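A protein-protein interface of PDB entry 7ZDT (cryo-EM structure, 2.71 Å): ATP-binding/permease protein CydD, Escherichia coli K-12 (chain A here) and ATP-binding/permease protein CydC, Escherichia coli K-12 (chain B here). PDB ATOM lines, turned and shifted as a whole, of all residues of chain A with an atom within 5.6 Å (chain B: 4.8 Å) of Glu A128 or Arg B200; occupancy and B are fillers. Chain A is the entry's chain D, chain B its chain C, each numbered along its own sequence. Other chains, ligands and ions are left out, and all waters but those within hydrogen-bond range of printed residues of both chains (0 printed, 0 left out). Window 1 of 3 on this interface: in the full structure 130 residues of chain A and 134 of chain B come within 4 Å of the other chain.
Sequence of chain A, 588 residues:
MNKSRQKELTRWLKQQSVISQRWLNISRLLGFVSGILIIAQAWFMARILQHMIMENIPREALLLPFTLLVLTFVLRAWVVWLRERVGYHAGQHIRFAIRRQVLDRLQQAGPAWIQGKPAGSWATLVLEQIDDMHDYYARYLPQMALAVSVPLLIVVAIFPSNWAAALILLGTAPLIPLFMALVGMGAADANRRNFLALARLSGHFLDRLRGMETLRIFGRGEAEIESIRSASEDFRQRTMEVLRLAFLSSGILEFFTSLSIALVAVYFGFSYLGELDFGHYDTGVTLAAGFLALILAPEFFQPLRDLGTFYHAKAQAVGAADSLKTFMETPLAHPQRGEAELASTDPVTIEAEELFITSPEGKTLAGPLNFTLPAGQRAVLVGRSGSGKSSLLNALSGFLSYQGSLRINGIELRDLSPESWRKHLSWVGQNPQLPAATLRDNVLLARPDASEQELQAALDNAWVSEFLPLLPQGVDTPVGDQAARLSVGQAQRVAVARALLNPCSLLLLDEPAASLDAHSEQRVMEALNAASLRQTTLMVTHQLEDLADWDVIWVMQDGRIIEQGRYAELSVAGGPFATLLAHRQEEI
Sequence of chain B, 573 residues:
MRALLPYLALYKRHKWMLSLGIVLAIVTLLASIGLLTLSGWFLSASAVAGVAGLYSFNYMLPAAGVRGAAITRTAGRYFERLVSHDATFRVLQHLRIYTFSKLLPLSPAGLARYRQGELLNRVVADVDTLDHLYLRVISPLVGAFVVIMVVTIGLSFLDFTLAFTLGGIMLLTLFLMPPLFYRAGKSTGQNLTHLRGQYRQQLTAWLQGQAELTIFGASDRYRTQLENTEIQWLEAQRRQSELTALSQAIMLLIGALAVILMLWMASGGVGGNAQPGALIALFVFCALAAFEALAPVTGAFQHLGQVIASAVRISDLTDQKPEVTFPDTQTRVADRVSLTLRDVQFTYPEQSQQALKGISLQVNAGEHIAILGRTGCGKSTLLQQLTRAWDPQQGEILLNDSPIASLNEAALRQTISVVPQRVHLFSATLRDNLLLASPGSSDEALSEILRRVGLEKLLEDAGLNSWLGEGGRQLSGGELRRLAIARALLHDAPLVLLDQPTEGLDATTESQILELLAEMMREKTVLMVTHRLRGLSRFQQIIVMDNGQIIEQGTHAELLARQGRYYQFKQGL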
ATOM      1  N   ALA A 123       6.392  -4.802 -27.703  1.00  0.00           N
ATOM      2  CA  ALA A 123       5.711  -3.984 -26.705  1.00  0.00           C
ATOM      3  C   ALA A 123       6.456  -3.992 -25.377  1.00  0.00           C
ATOM      4  O   ALA A 123       6.494  -2.977 -24.674  1.00  0.00           O
ATOM      5  CB  ALA A 123       4.276  -4.474 -26.519  1.00  0.00           C
ATOM      6  N   THR A 124       7.042  -5.131 -25.012  1.00  0.00           N
ATOM      7  CA  THR A 124       7.877  -5.185 -23.817  1.00  0.00           C
ATOM      8  C   THR A 124       9.116  -4.318 -23.985  1.00  0.00           C
ATOM      9  O   THR A 124       9.547  -3.636 -23.050  1.00  0.00           O
ATOM     10  CB  THR A 124       8.261  -6.635 -23.518  1.00  0.00           C
ATOM     11  OG1 THR A 124       7.095  -7.359 -23.110  1.00  0.00           O
ATOM     12  CG2 THR A 124       9.300  -6.704 -22.415  1.00  0.00           C
ATOM     13  N   LEU A 125       9.696  -4.329 -25.183  1.00  0.00           N
ATOM     14  CA  LEU A 125      10.871  -3.512 -25.465  1.00  0.00           C
ATOM     15  C   LEU A 125      10.557  -2.026 -25.348  1.00  0.00           C
ATOM     16  O   LEU A 125      11.360  -1.251 -24.819  1.00  0.00           O
ATOM     17  CB  LEU A 125      11.401  -3.852 -26.855  1.00  0.00           C
ATOM     18  CG  LEU A 125      12.632  -3.132 -27.394  1.00  0.00           C
ATOM     19  CD1 LEU A 125      13.570  -4.122 -28.034  1.00  0.00           C
ATOM     20  CD2 LEU A 125      12.203  -2.101 -28.412  1.00  0.00           C
ATOM     21  N   VAL A 126       9.386  -1.613 -25.831  1.00  0.00           N
ATOM     22  CA  VAL A 126       9.074  -0.188 -25.911  1.00  0.00           C
ATOM     23  C   VAL A 126       8.493   0.309 -24.591  1.00  0.00           C
ATOM     24  O   VAL A 126       8.772   1.432 -24.157  1.00  0.00           O
ATOM     25  CB  VAL A 126       8.123   0.082 -27.091  1.00  0.00           C
ATOM     26  CG1 VAL A 126       7.671   1.527 -27.103  1.00  0.00           C
ATOM     27  CG2 VAL A 126       8.797  -0.276 -28.397  1.00  0.00           C
ATOM     28  N   LEU A 127       7.682  -0.517 -23.927  1.00  0.00           N
ATOM     29  CA  LEU A 127       7.013  -0.060 -22.713  1.00  0.00           C
ATOM     30  C   LEU A 127       7.796  -0.440 -21.462  1.00  0.00           C
ATOM     31  O   LEU A 127       8.190   0.431 -20.683  1.00  0.00           O
ATOM     32  CB  LEU A 127       5.594  -0.626 -22.639  1.00  0.00           C
ATOM     33  CG  LEU A 127       4.478   0.127 -23.360  1.00  0.00           C
ATOM     34  CD1 LEU A 127       4.486  -0.183 -24.839  1.00  0.00           C
ATOM     35  CD2 LEU A 127       3.130  -0.198 -22.757  1.00  0.00           C
ATOM     36  N   GLU A 128       8.024  -1.736 -21.250  1.00  0.00           N
ATOM     37  CA  GLU A 128       8.588  -2.188 -19.982  1.00  0.00           C
ATOM     38  C   GLU A 128      10.064  -1.835 -19.853  1.00  0.00           C
ATOM     39  O   GLU A 128      10.513  -1.430 -18.778  1.00  0.00           O
ATOM     40  CB  GLU A 128       8.402  -3.695 -19.827  1.00  0.00           C
ATOM     41  CG  GLU A 128       7.116  -4.118 -19.150  1.00  0.00           C
ATOM     42  CD  GLU A 128       5.989  -4.355 -20.129  1.00  0.00           C
ATOM     43  OE1 GLU A 128       6.139  -3.992 -21.312  1.00  0.00           O
ATOM     44  OE2 GLU A 128       4.962  -4.932 -19.718  1.00  0.00           O
ATOM     45  N   GLN A 129      10.839  -2.001 -20.924  1.00  0.00           N
ATOM     46  CA  GLN A 129      12.282  -1.839 -20.828  1.00  0.00           C
ATOM     47  C   GLN A 129      12.738  -0.390 -20.887  1.00  0.00           C
ATOM     48  O   GLN A 129      13.736  -0.050 -20.247  1.00  0.00           O
ATOM     49  CB  GLN A 129      12.987  -2.637 -21.925  1.00  0.00           C
ATOM     50  CG  GLN A 129      12.731  -4.125 -21.860  1.00  0.00           C
ATOM     51  CD  GLN A 129      13.479  -4.888 -22.924  1.00  0.00           C
ATOM     52  OE1 GLN A 129      14.539  -4.463 -23.375  1.00  0.00           O
ATOM     53  NE2 GLN A 129      12.935  -6.026 -23.332  1.00  0.00           N
ATOM     54  N   ILE A 130      12.049   0.472 -21.637  1.00  0.00           N
ATOM     55  CA  ILE A 130      12.361   1.897 -21.592  1.00  0.00           C
ATOM     56  C   ILE A 130      11.898   2.543 -20.295  1.00  0.00           C
ATOM     57  O   ILE A 130      12.599   3.418 -19.766  1.00  0.00           O
ATOM     58  CB  ILE A 130      11.763   2.635 -22.805  1.00  0.00           C
ATOM     59  CG1 ILE A 130      12.366   2.093 -24.098  1.00  0.00           C
ATOM     60  CG2 ILE A 130      12.019   4.126 -22.712  1.00  0.00           C
ATOM     61  CD1 ILE A 130      11.803   2.723 -25.338  1.00  0.00           C
ATOM     62  N   ASP A 131      10.758   2.125 -19.748  1.00  0.00           N
ATOM     63  CA  ASP A 131      10.268   2.670 -18.491  1.00  0.00           C
ATOM     64  C   ASP A 131      11.088   2.245 -17.287  1.00  0.00           C
ATOM     65  O   ASP A 131      11.104   2.969 -16.287  1.00  0.00           O
ATOM     66  CB  ASP A 131       8.812   2.263 -18.261  1.00  0.00           C
ATOM     67  CG  ASP A 131       7.835   3.303 -18.749  1.00  0.00           C
ATOM     68  OD1 ASP A 131       8.284   4.346 -19.265  1.00  0.00           O
ATOM     69  OD2 ASP A 131       6.615   3.082 -18.610  1.00  0.00           O
ATOM     70  N   ASP A 132      11.762   1.103 -17.351  1.00  0.00           N
ATOM     71  CA  ASP A 132      12.577   0.626 -16.246  1.00  0.00           C
ATOM     72  C   ASP A 132      13.969   1.242 -16.240  1.00  0.00           C
ATOM     73  O   ASP A 132      14.790   0.888 -15.390  1.00  0.00           O
ATOM     74  CB  ASP A 132      12.669  -0.899 -16.273  1.00  0.00           C
ATOM     75  CG  ASP A 132      11.435  -1.563 -15.695  1.00  0.00           C
ATOM     76  OD1 ASP A 132      10.699  -0.890 -14.945  1.00  0.00           O
ATOM     77  OD2 ASP A 132      11.200  -2.754 -15.980  1.00  0.00           O
ATOM     78  N   MET A 133      14.247   2.151 -17.167  1.00  0.00           N
ATOM     79  CA  MET A 133      15.455   2.957 -17.144  1.00  0.00           C
ATOM     80  C   MET A 133      15.309   4.212 -16.302  1.00  0.00           C
ATOM     81  O   MET A 133      16.301   4.916 -16.101  1.00  0.00           O
ATOM     82  CB  MET A 133      15.846   3.365 -18.562  1.00  0.00           C
ATOM     83  CG  MET A 133      16.082   2.221 -19.499  1.00  0.00           C
ATOM     84  SD  MET A 133      16.484   2.812 -21.141  1.00  0.00           S
ATOM     85  CE  MET A 133      17.282   1.363 -21.797  1.00  0.00           C
ATOM     86  N   PHE A 195      14.125  -9.490 -18.491  1.00  0.00           N
ATOM     87  CA  PHE A 195      13.437  -8.884 -19.624  1.00  0.00           C
ATOM     88  C   PHE A 195      13.340  -9.845 -20.798  1.00  0.00           C
ATOM     89  O   PHE A 195      12.408  -9.747 -21.603  1.00  0.00           O
ATOM     90  CB  PHE A 195      14.156  -7.606 -20.046  1.00  0.00           C
ATOM     91  CG  PHE A 195      14.001  -6.477 -19.078  1.00  0.00           C
ATOM     92  CD1 PHE A 195      12.752  -5.952 -18.802  1.00  0.00           C
ATOM     93  CD2 PHE A 195      15.101  -5.941 -18.439  1.00  0.00           C
ATOM     94  CE1 PHE A 195      12.609  -4.916 -17.916  1.00  0.00           C
ATOM     95  CE2 PHE A 195      14.959  -4.906 -17.546  1.00  0.00           C
ATOM     96  CZ  PHE A 195      13.715  -4.392 -17.287  1.00  0.00           C
ATOM     97  N   LEU A 198      10.348 -11.880 -19.925  1.00  0.00           N
ATOM     98  CA  LEU A 198       9.122 -11.102 -20.033  1.00  0.00           C
ATOM     99  C   LEU A 198       8.737 -10.865 -21.485  1.00  0.00           C
ATOM    100  O   LEU A 198       7.551 -10.922 -21.826  1.00  0.00           O
ATOM    101  CB  LEU A 198       9.284  -9.771 -19.303  1.00  0.00           C
ATOM    102  CG  LEU A 198       8.168  -8.744 -19.460  1.00  0.00           C
ATOM    103  CD1 LEU A 198       6.851  -9.290 -18.950  1.00  0.00           C
ATOM    104  CD2 LEU A 198       8.537  -7.474 -18.737  1.00  0.00           C
ATOM    105  N   SER A 202       5.399 -12.281 -23.120  1.00  0.00           N
ATOM    106  CA  SER A 202       4.472 -11.365 -23.776  1.00  0.00           C
ATOM    107  C   SER A 202       4.303 -11.708 -25.251  1.00  0.00           C
ATOM    108  O   SER A 202       3.188 -11.668 -25.777  1.00  0.00           O
ATOM    109  CB  SER A 202       4.957  -9.930 -23.615  1.00  0.00           C
ATOM    110  OG  SER A 202       4.774  -9.486 -22.286  1.00  0.00           O
ATOM    111  N   GLY B 117      -4.304  -5.950 -28.142  1.00  0.00           N
ATOM    112  CA  GLY B 117      -3.251  -5.320 -27.366  1.00  0.00           C
ATOM    113  C   GLY B 117      -3.665  -4.941 -25.963  1.00  0.00           C
ATOM    114  O   GLY B 117      -2.807  -4.841 -25.082  1.00  0.00           O
ATOM    115  N   LEU B 120      -3.555  -8.262 -24.027  1.00  0.00           N
ATOM    116  CA  LEU B 120      -2.169  -8.497 -23.646  1.00  0.00           C
ATOM    117  C   LEU B 120      -1.776  -7.662 -22.440  1.00  0.00           C
ATOM    118  O   LEU B 120      -1.035  -8.137 -21.576  1.00  0.00           O
ATOM    119  CB  LEU B 120      -1.254  -8.213 -24.838  1.00  0.00           C
ATOM    120  CG  LEU B 120       0.237  -7.980 -24.602  1.00  0.00           C
ATOM    121  CD1 LEU B 120       0.912  -9.255 -24.157  1.00  0.00           C
ATOM    122  CD2 LEU B 120       0.886  -7.454 -25.862  1.00  0.00           C
ATOM    123  N   ASN B 121      -2.273  -6.428 -22.353  1.00  0.00           N
ATOM    124  CA  ASN B 121      -1.951  -5.573 -21.217  1.00  0.00           C
ATOM    125  C   ASN B 121      -2.525  -6.112 -19.912  1.00  0.00           C
ATOM    126  O   ASN B 121      -1.944  -5.891 -18.847  1.00  0.00           O
ATOM    127  CB  ASN B 121      -2.462  -4.156 -21.470  1.00  0.00           C
ATOM    128  CG  ASN B 121      -1.769  -3.129 -20.609  1.00  0.00           C
ATOM    129  OD1 ASN B 121      -0.598  -2.825 -20.811  1.00  0.00           O
ATOM    130  ND2 ASN B 121      -2.489  -2.591 -19.637  1.00  0.00           N
ATOM    131  N   VAL B 124      -0.304  -9.592 -18.605  1.00  0.00           N
ATOM    132  CA  VAL B 124       1.095  -9.419 -18.237  1.00  0.00           C
ATOM    133  C   VAL B 124       1.311  -8.144 -17.426  1.00  0.00           C
ATOM    134  O   VAL B 124       2.042  -8.149 -16.437  1.00  0.00           O
ATOM    135  CB  VAL B 124       2.017  -9.461 -19.480  1.00  0.00           C
ATOM    136  CG1 VAL B 124       1.813 -10.754 -20.250  1.00  0.00           C
ATOM    137  CG2 VAL B 124       1.812  -8.256 -20.388  1.00  0.00           C
ATOM    138  N   ALA B 125       0.670  -7.044 -17.819  1.00  0.00           N
ATOM    139  CA  ALA B 125       0.947  -5.760 -17.188  1.00  0.00           C
ATOM    140  C   ALA B 125      -0.011  -5.439 -16.051  1.00  0.00           C
ATOM    141  O   ALA B 125       0.411  -4.895 -15.028  1.00  0.00           O
ATOM    142  CB  ALA B 125       0.905  -4.643 -18.232  1.00  0.00           C
ATOM    143  N   ARG B 196      -1.896   3.217 -20.188  1.00  0.00           N
ATOM    144  CA  ARG B 196      -0.872   2.233 -20.521  1.00  0.00           C
ATOM    145  C   ARG B 196      -1.436   1.135 -21.410  1.00  0.00           C
ATOM    146  O   ARG B 196      -0.755   0.655 -22.323  1.00  0.00           O
ATOM    147  CB  ARG B 196      -0.274   1.628 -19.258  1.00  0.00           C
ATOM    148  CG  ARG B 196       0.756   0.555 -19.554  1.00  0.00           C
ATOM    149  CD  ARG B 196       1.381  -0.006 -18.302  1.00  0.00           C
ATOM    150  NE  ARG B 196       0.387  -0.611 -17.428  1.00  0.00           N
ATOM    151  CZ  ARG B 196       0.678  -1.261 -16.310  1.00  0.00           C
ATOM    152  NH1 ARG B 196       1.940  -1.391 -15.933  1.00  0.00           N
ATOM    153  NH2 ARG B 196      -0.292  -1.781 -15.571  1.00  0.00           N
ATOM    154  N   GLY B 197      -2.677   0.715 -21.158  1.00  0.00           N
ATOM    155  CA  GLY B 197      -3.292  -0.288 -22.005  1.00  0.00           C
ATOM    156  C   GLY B 197      -3.713   0.248 -23.349  1.00  0.00           C
ATOM    157  O   GLY B 197      -3.733  -0.494 -24.335  1.00  0.00           O
ATOM    158  N   GLN B 198      -4.065   1.532 -23.414  1.00  0.00           N
ATOM    159  CA  GLN B 198      -4.355   2.158 -24.698  1.00  0.00           C
ATOM    160  C   GLN B 198      -3.094   2.342 -25.523  1.00  0.00           C
ATOM    161  O   GLN B 198      -3.138   2.234 -26.752  1.00  0.00           O
ATOM    162  CB  GLN B 198      -5.050   3.499 -24.480  1.00  0.00           C
ATOM    163  CG  GLN B 198      -5.642   4.091 -25.739  1.00  0.00           C
ATOM    164  CD  GLN B 198      -6.098   5.518 -25.555  1.00  0.00           C
ATOM    165  OE1 GLN B 198      -5.298   6.405 -25.272  1.00  0.00           O
ATOM    166  NE2 GLN B 198      -7.392   5.747 -25.715  1.00  0.00           N
ATOM    167  N   TYR B 199      -1.965   2.623 -24.871  1.00  0.00           N
ATOM    168  CA  TYR B 199      -0.704   2.746 -25.590  1.00  0.00           C
ATOM    169  C   TYR B 199      -0.248   1.404 -26.145  1.00  0.00           C
ATOM    170  O   TYR B 199       0.249   1.330 -27.272  1.00  0.00           O
ATOM    171  CB  TYR B 199       0.367   3.342 -24.677  1.00  0.00           C
ATOM    172  CG  TYR B 199       1.623   3.732 -25.414  1.00  0.00           C
ATOM    173  CD1 TYR B 199       1.724   4.962 -26.037  1.00  0.00           C
ATOM    174  CD2 TYR B 199       2.699   2.865 -25.504  1.00  0.00           C
ATOM    175  CE1 TYR B 199       2.859   5.322 -26.717  1.00  0.00           C
ATOM    176  CE2 TYR B 199       3.839   3.217 -26.190  1.00  0.00           C
ATOM    177  CZ  TYR B 199       3.911   4.448 -26.792  1.00  0.00           C
ATOM    178  OH  TYR B 199       5.042   4.817 -27.474  1.00  0.00           O
ATOM    179  N   ARG B 200      -0.406   0.330 -25.370  1.00  0.00           N
ATOM    180  CA  ARG B 200       0.008  -0.987 -25.837  1.00  0.00           C
ATOM    181  C   ARG B 200      -0.879  -1.491 -26.968  1.00  0.00           C
ATOM    182  O   ARG B 200      -0.396  -2.191 -27.861  1.00  0.00           O
ATOM    183  CB  ARG B 200       0.014  -1.984 -24.680  1.00  0.00           C
ATOM    184  CG  ARG B 200       0.707  -3.294 -25.014  1.00  0.00           C
ATOM    185  CD  ARG B 200       0.675  -4.275 -23.861  1.00  0.00           C
ATOM    186  NE  ARG B 200       0.959  -3.640 -22.578  1.00  0.00           N
ATOM    187  CZ  ARG B 200       2.157  -3.609 -22.008  1.00  0.00           C
ATOM    188  NH1 ARG B 200       3.193  -4.173 -22.609  1.00  0.00           N
ATOM    189  NH2 ARG B 200       2.322  -3.010 -20.839  1.00  0.00           N
ATOM    190  N   GLN B 201      -2.173  -1.170 -26.943  1.00  0.00           N
ATOM    191  CA  GLN B 201      -3.039  -1.548 -28.052  1.00  0.00           C
ATOM    192  C   GLN B 201      -2.690  -0.768 -29.313  1.00  0.00           C
ATOM    193  O   GLN B 201      -2.594  -1.348 -30.400  1.00  0.00           O
ATOM    194  CB  GLN B 201      -4.503  -1.338 -27.674  1.00  0.00           C
ATOM    195  CG  GLN B 201      -5.466  -1.313 -28.850  1.00  0.00           C
ATOM    196  CD  GLN B 201      -5.440  -2.588 -29.676  1.00  0.00           C
ATOM    197  OE1 GLN B 201      -5.257  -3.681 -29.147  1.00  0.00           O
ATOM    198  NE2 GLN B 201      -5.631  -2.451 -30.979  1.00  0.00           N
ATOM    199  N   GLN B 202      -2.483   0.542 -29.188  1.00  0.00           N
ATOM    200  CA  GLN B 202      -2.144   1.345 -30.356  1.00  0.00           C
ATOM    201  C   GLN B 202      -0.778   0.978 -30.915  1.00  0.00           C
ATOM    202  O   GLN B 202      -0.575   1.040 -32.129  1.00  0.00           O
ATOM    203  CB  GLN B 202      -2.187   2.832 -30.012  1.00  0.00           C
ATOM    204  CG  GLN B 202      -3.572   3.378 -29.775  1.00  0.00           C
ATOM    205  CD  GLN B 202      -3.546   4.818 -29.334  1.00  0.00           C
ATOM    206  OE1 GLN B 202      -2.511   5.326 -28.918  1.00  0.00           O
ATOM    207  NE2 GLN B 202      -4.688   5.484 -29.411  1.00  0.00           N
ATOM    208  N   LEU B 203       0.169   0.604 -30.054  1.00  0.00           N
ATOM    209  CA  LEU B 203       1.503   0.253 -30.534  1.00  0.00           C
ATOM    210  C   LEU B 203       1.499  -1.089 -31.253  1.00  0.00           C
ATOM    211  O   LEU B 203       2.126  -1.233 -32.307  1.00  0.00           O
ATOM    212  CB  LEU B 203       2.492   0.234 -29.372  1.00  0.00           C
ATOM    213  CG  LEU B 203       3.857  -0.385 -29.667  1.00  0.00           C
ATOM    214  CD1 LEU B 203       4.773   0.616 -30.339  1.00  0.00           C
ATOM    215  CD2 LEU B 203       4.479  -0.918 -28.400  1.00  0.00           C
ATOM    216  N   THR B 204       0.803  -2.084 -30.701  1.00  0.00           N
ATOM    217  CA  THR B 204       0.732  -3.384 -31.358  1.00  0.00           C
ATOM    218  C   THR B 204      -0.052  -3.303 -32.660  1.00  0.00           C
ATOM    219  O   THR B 204       0.314  -3.940 -33.651  1.00  0.00           O
ATOM    220  CB  THR B 204       0.113  -4.419 -30.422  1.00  0.00           C
ATOM    221  OG1 THR B 204      -1.108  -3.906 -29.879  1.00  0.00           O
ATOM    222  CG2 THR B 204       1.067  -4.752 -29.291  1.00  0.00           C
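NH1 of Arg B200 lies within salt-bridge range of OE1 of Glu A128 (3.2 Å).
OD1 of Asn B121 is in hydrogen-bond range of NE of Arg B200 (2.5 Å). The backbone carbonyl oxygen of Arg B200 lies within hydrogen-bond range of the side-chain hydroxyl of Thr B204 (2.7 Å). The side-chain hydroxyl of Ser A202 is in hydrogen-bond range of the backbone carbonyl oxygen of Leu A198 (3.2 Å). The side-chain hydroxyl (OG1) of Thr A124 is in hydrogen-bond range of the side-chain hydroxyl (OG) of Ser A202, at 3.3 Å.
CA of Ala A123 touches CD2 of Leu B203, 3.7 Å away. Val A126 touches Leu B203. Leu A127 touches Tyr B199 (CD1 to CD2, 3.6 Å). Leu A127 touches Arg B200. Leu A127 touches Leu B203. Leu B120 touches Ser A202. CG2 of Val B124 touches OG of Ser A202, 3.7 Å away.
Of the printed residues of chain B, Ala A123 touches Leu B203 (3.7 Å). Of the printed residues of chain B, Val A126 touches Leu B203. Glu A128 touches just one residue of chain B: Arg B200. Gln A129 touches none of the printed residues of chain B. Of the printed residues of chain A, Leu B120 touches Ser A202. Arg B196 touches none of the printed residues of chain A. Arg B200 touches just these residues of chain A: Leu A127 and Glu A128. The nearest residue of chain B that does not touch Glu A128 is Ala B125 (4.3 Å). The nearest residue of chain A that does not touch Arg B200 is Ala A123 (4.05 Å).
Hydrophobic or aromatic side chains of chain A that line the printed part of chain B: Val A126 and Leu A127. Hydrophobic or aromatic side chains of chain B within 4 Å of the printed part of chain A: Leu B120, Val B124, Tyr B199 and Leu B203. Along chain B the printed residues that touch a printed residue of chain A span positions 120 to 203.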
